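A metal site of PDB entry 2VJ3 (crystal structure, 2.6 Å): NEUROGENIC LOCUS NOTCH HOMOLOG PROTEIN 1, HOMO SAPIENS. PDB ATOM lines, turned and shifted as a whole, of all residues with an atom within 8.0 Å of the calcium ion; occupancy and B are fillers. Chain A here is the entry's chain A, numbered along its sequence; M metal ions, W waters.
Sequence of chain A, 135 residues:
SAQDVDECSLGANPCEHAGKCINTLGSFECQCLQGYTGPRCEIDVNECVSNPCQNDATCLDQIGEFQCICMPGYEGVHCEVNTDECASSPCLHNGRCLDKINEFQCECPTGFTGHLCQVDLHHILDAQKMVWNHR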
ATOM      1  N   GLN A  34     -34.826 -12.229  -6.869  1.00  0.00           N
ATOM      2  CA  GLN A  34     -33.751 -12.839  -7.643  1.00  0.00           C
ATOM      3  C   GLN A  34     -32.418 -12.110  -7.442  1.00  0.00           C
ATOM      4  O   GLN A  34     -32.306 -10.922  -7.747  1.00  0.00           O
ATOM      5  CB  GLN A  34     -34.124 -12.898  -9.130  1.00  0.00           C
ATOM      6  CG  GLN A  34     -33.290 -13.857  -9.959  1.00  0.00           C
ATOM      7  CD  GLN A  34     -33.779 -15.295  -9.931  1.00  0.00           C
ATOM      8  OE1 GLN A  34     -34.127 -15.827  -8.879  1.00  0.00           O
ATOM      9  NE2 GLN A  34     -33.817 -15.934 -11.087  1.00  0.00           N
ATOM     10  N   GLY A  35     -31.432 -12.832  -6.904  1.00  0.00           N
ATOM     11  CA  GLY A  35     -30.109 -12.271  -6.649  1.00  0.00           C
ATOM     12  C   GLY A  35     -29.788 -12.052  -5.189  1.00  0.00           C
ATOM     13  O   GLY A  35     -28.703 -11.573  -4.851  1.00  0.00           O
ATOM     14  N   TYR A  36     -30.735 -12.410  -4.322  1.00  0.00           N
ATOM     15  CA  TYR A  36     -30.550 -12.278  -2.877  1.00  0.00           C
ATOM     16  C   TYR A  36     -30.844 -13.596  -2.162  1.00  0.00           C
ATOM     17  O   TYR A  36     -31.783 -14.308  -2.525  1.00  0.00           O
ATOM     18  CB  TYR A  36     -31.419 -11.157  -2.314  1.00  0.00           C
ATOM     19  CG  TYR A  36     -31.168  -9.805  -2.946  1.00  0.00           C
ATOM     20  CD1 TYR A  36     -30.036  -9.064  -2.627  1.00  0.00           C
ATOM     21  CD2 TYR A  36     -32.083  -9.266  -3.861  1.00  0.00           C
ATOM     22  CE1 TYR A  36     -29.797  -7.820  -3.206  1.00  0.00           C
ATOM     23  CE2 TYR A  36     -31.852  -8.023  -4.446  1.00  0.00           C
ATOM     24  CZ  TYR A  36     -30.715  -7.300  -4.111  1.00  0.00           C
ATOM     25  OH  TYR A  36     -30.487  -6.078  -4.687  1.00  0.00           O
ATOM     26  N   ILE A  43     -27.854 -11.378   1.960  1.00  0.00           N
ATOM     27  CA  ILE A  43     -26.705 -11.658   1.111  1.00  0.00           C
ATOM     28  C   ILE A  43     -26.984 -11.273  -0.340  1.00  0.00           C
ATOM     29  O   ILE A  43     -27.905 -11.794  -0.976  1.00  0.00           O
ATOM     30  CB  ILE A  43     -26.290 -13.156   1.153  1.00  0.00           C
ATOM     31  CG1 ILE A  43     -25.907 -13.577   2.576  1.00  0.00           C
ATOM     32  CG2 ILE A  43     -25.139 -13.423   0.174  1.00  0.00           C
ATOM     33  CD1 ILE A  43     -25.548 -15.043   2.702  1.00  0.00           C
ATOM     34  N   ASP A  44     -26.169 -10.348  -0.862  1.00  0.00           N
ATOM     35  CA  ASP A  44     -26.157 -10.051  -2.289  1.00  0.00           C
ATOM     36  C   ASP A  44     -25.264 -11.071  -2.962  1.00  0.00           C
ATOM     37  O   ASP A  44     -24.031 -10.973  -2.898  1.00  0.00           O
ATOM     38  CB  ASP A  44     -25.663  -8.623  -2.538  1.00  0.00           C
ATOM     39  CG  ASP A  44     -25.745  -8.213  -3.991  1.00  0.00           C
ATOM     40  OD1 ASP A  44     -26.462  -8.873  -4.782  1.00  0.00           O
ATOM     41  OD2 ASP A  44     -25.071  -7.230  -4.356  1.00  0.00           O
ATOM     42  N   VAL A  45     -25.882 -12.070  -3.594  1.00  0.00           N
ATOM     43  CA  VAL A  45     -25.179 -13.179  -4.221  1.00  0.00           C
ATOM     44  C   VAL A  45     -24.107 -12.669  -5.190  1.00  0.00           C
ATOM     45  O   VAL A  45     -24.394 -11.881  -6.086  1.00  0.00           O
ATOM     46  CB  VAL A  45     -26.145 -14.135  -4.982  1.00  0.00           C
ATOM     47  CG1 VAL A  45     -25.405 -15.341  -5.540  1.00  0.00           C
ATOM     48  CG2 VAL A  45     -27.269 -14.582  -4.084  1.00  0.00           C
ATOM     49  N   ASN A  46     -22.870 -13.125  -4.986  1.00  0.00           N
ATOM     50  CA  ASN A  46     -21.773 -12.775  -5.882  1.00  0.00           C
ATOM     51  C   ASN A  46     -21.722 -13.739  -7.059  1.00  0.00           C
ATOM     52  O   ASN A  46     -21.241 -14.865  -6.926  1.00  0.00           O
ATOM     53  CB  ASN A  46     -20.439 -12.758  -5.124  1.00  0.00           C
ATOM     54  CG  ASN A  46     -19.327 -12.047  -5.881  1.00  0.00           C
ATOM     55  OD1 ASN A  46     -19.444 -11.772  -7.076  1.00  0.00           O
ATOM     56  ND2 ASN A  46     -18.234 -11.742  -5.181  1.00  0.00           N
ATOM     57  N   GLU A  47     -22.231 -13.293  -8.206  1.00  0.00           N
ATOM     58  CA  GLU A  47     -22.251 -14.110  -9.415  1.00  0.00           C
ATOM     59  C   GLU A  47     -20.875 -14.151 -10.090  1.00  0.00           C
ATOM     60  O   GLU A  47     -20.696 -14.824 -11.110  1.00  0.00           O
ATOM     61  CB  GLU A  47     -23.316 -13.607 -10.395  1.00  0.00           C
ATOM     62  CG  GLU A  47     -24.756 -13.967 -10.007  1.00  0.00           C
ATOM     63  CD  GLU A  47     -25.391 -12.973  -9.044  1.00  0.00           C
ATOM     64  OE1 GLU A  47     -24.824 -11.879  -8.839  1.00  0.00           O
ATOM     65  OE2 GLU A  47     -26.474 -13.279  -8.506  1.00  0.00           O
ATOM     66  N   CYS A  48     -19.919 -13.437  -9.514  1.00  0.00           N
ATOM     67  CA  CYS A  48     -18.546 -13.382 -10.017  1.00  0.00           C
ATOM     68  C   CYS A  48     -17.570 -14.159  -9.120  1.00  0.00           C
ATOM     69  O   CYS A  48     -16.367 -14.174  -9.387  1.00  0.00           O
ATOM     70  CB  CYS A  48     -18.088 -11.932 -10.138  1.00  0.00           C
ATOM     71  SG  CYS A  48     -18.970 -10.995 -11.401  1.00  0.00           S
ATOM     72  N   LEU A  60     -18.796  -8.190 -13.663  1.00  0.00           N
ATOM     73  CA  LEU A  60     -19.653  -7.217 -12.999  1.00  0.00           C
ATOM     74  C   LEU A  60     -20.661  -7.932 -12.111  1.00  0.00           C
ATOM     75  O   LEU A  60     -21.536  -8.648 -12.591  1.00  0.00           O
ATOM     76  CB  LEU A  60     -20.383  -6.342 -14.026  1.00  0.00           C
ATOM     77  CG  LEU A  60     -19.544  -5.472 -14.977  1.00  0.00           C
ATOM     78  CD1 LEU A  60     -20.397  -4.998 -16.144  1.00  0.00           C
ATOM     79  CD2 LEU A  60     -18.899  -4.293 -14.267  1.00  0.00           C
ATOM     80  N   ASP A  61     -20.513  -7.734 -10.803  1.00  0.00           N
ATOM     81  CA  ASP A  61     -21.411  -8.323  -9.818  1.00  0.00           C
ATOM     82  C   ASP A  61     -22.728  -7.540  -9.780  1.00  0.00           C
ATOM     83  O   ASP A  61     -22.806  -6.474  -9.168  1.00  0.00           O
ATOM     84  CB  ASP A  61     -20.751  -8.361  -8.440  1.00  0.00           C
ATOM     85  CG  ASP A  61     -21.502  -9.219  -7.438  1.00  0.00           C
ATOM     86  OD1 ASP A  61     -22.406  -9.981  -7.837  1.00  0.00           O
ATOM     87  OD2 ASP A  61     -21.192  -9.139  -6.229  1.00  0.00           O
ATOM     88  N   GLN A  62     -23.737  -8.071 -10.451  1.00  0.00           N
ATOM     89  CA  GLN A  62     -25.026  -7.412 -10.604  1.00  0.00           C
ATOM     90  C   GLN A  62     -26.129  -8.128  -9.825  1.00  0.00           C
ATOM     91  O   GLN A  62     -25.880  -9.180  -9.231  1.00  0.00           O
ATOM     92  CB  GLN A  62     -25.396  -7.315 -12.087  1.00  0.00           C
ATOM     93  CG  GLN A  62     -24.436  -6.456 -12.908  1.00  0.00           C
ATOM     94  CD  GLN A  62     -24.541  -6.703 -14.404  1.00  0.00           C
ATOM     95  OE1 GLN A  62     -25.470  -7.356 -14.876  1.00  0.00           O
ATOM     96  NE2 GLN A  62     -23.599  -6.164 -15.141  1.00  0.00           N
ATOM     97  N   ILE A  63     -27.326  -7.553  -9.820  1.00  0.00           N
ATOM     98  CA  ILE A  63     -28.471  -8.132  -9.101  1.00  0.00           C
ATOM     99  C   ILE A  63     -29.052  -9.300  -9.889  1.00  0.00           C
ATOM    100  O   ILE A  63     -29.763  -9.115 -10.885  1.00  0.00           O
ATOM    101  CB  ILE A  63     -29.559  -7.075  -8.795  1.00  0.00           C
ATOM    102  CG1 ILE A  63     -28.951  -5.878  -8.049  1.00  0.00           C
ATOM    103  CG2 ILE A  63     -30.697  -7.690  -7.979  1.00  0.00           C
ATOM    104  CD1 ILE A  63     -29.756  -4.585  -8.181  1.00  0.00           C
ATOM    105  N   GLY A  64     -28.752 -10.516  -9.438  1.00  0.00           N
ATOM    106  CA  GLY A  64     -29.272 -11.740 -10.042  1.00  0.00           C
ATOM    107  C   GLY A  64     -28.565 -12.198 -11.304  1.00  0.00           C
ATOM    108  O   GLY A  64     -29.006 -13.147 -11.953  1.00  0.00           O
ATOM    109  N   GLU A  65     -27.454 -11.531 -11.639  1.00  0.00           N
ATOM    110  CA  GLU A  65     -26.708 -11.823 -12.864  1.00  0.00           C
ATOM    111  C   GLU A  65     -25.257 -11.348 -12.803  1.00  0.00           C
ATOM    112  O   GLU A  65     -24.866 -10.618 -11.897  1.00  0.00           O
ATOM    113  CB  GLU A  65     -27.405 -11.237 -14.092  1.00  0.00           C
ATOM    114  CG  GLU A  65     -27.621  -9.720 -14.041  1.00  0.00           C
ATOM    115  CD  GLU A  65     -28.150  -9.146 -15.349  1.00  0.00           C
ATOM    116  OE1 GLU A  65     -28.129  -9.859 -16.375  1.00  0.00           O
ATOM    117  OE2 GLU A  65     -28.578  -7.971 -15.342  1.00  0.00           O
ATOM    118  N   PHE A  66     -24.467 -11.784 -13.794  1.00  0.00           N
ATOM    119  CA  PHE A  66     -23.136 -11.258 -14.021  1.00  0.00           C
ATOM    120  C   PHE A  66     -22.991 -10.870 -15.476  1.00  0.00           C
ATOM    121  O   PHE A  66     -23.693 -11.404 -16.344  1.00  0.00           O
ATOM    122  CB  PHE A  66     -22.065 -12.290 -13.614  1.00  0.00           C
ATOM    123  CG  PHE A  66     -21.958 -13.467 -14.547  1.00  0.00           C
ATOM    124  CD1 PHE A  66     -22.745 -14.598 -14.362  1.00  0.00           C
ATOM    125  CD2 PHE A  66     -21.072 -13.446 -15.619  1.00  0.00           C
ATOM    126  CE1 PHE A  66     -22.647 -15.685 -15.222  1.00  0.00           C
ATOM    127  CE2 PHE A  66     -20.970 -14.522 -16.488  1.00  0.00           C
ATOM    128  CZ  PHE A  66     -21.756 -15.651 -16.288  1.00  0.00           C
HETATM  129 CA    CA M   1     -24.984  -9.874  -7.117  1.00  0.00          CA
HETATM  130  O   HOH W   1     -25.082  -7.458  -6.949  1.00  0.00           O
HETATM  131  O   HOH W   2     -27.198 -10.694  -6.680  1.00  0.00           O
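The backbone NH (N) of Val 45 sits at hydrogen-bond distance from the backbone carbonyl oxygen (O) of Gly 35 (3.1 Å).
OE1 of Gln 62 lies close to OE2 of Glu 65, at 3.2 Å.
The side-chain carboxylate of Asp 61 lies close to the side-chain amide oxygen of Asn 46 (3.3 Å).
The backbone NH (N) of Asp 61 lies within hydrogen-bond range of the side-chain sulfur (SG) of Cys 48, 3.7 Å away.
Five residues have an atom within 4 Å of the calcium ion: Asp 44, Val 45, Glu 47, Asp 61 and Gln 62.
The nearest printed residue that does not touch the calcium ion is Ile 63 (4.3 Å).
The calcium ion is bound by O of Val 45, O of Gln 62, water W2, water W1, OE1 of Glu 47 and OD1 of Asp 61.
Slightly farther from the calcium ion lies OD1 of Asp 44 (2.9 Å).
Water W1 lies within hydrogen-bond range of the side-chain carboxylate (OD2) of Asp 44 (2.6 Å) and the backbone carbonyl oxygen (O) of Asp 61 (3.3 Å).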
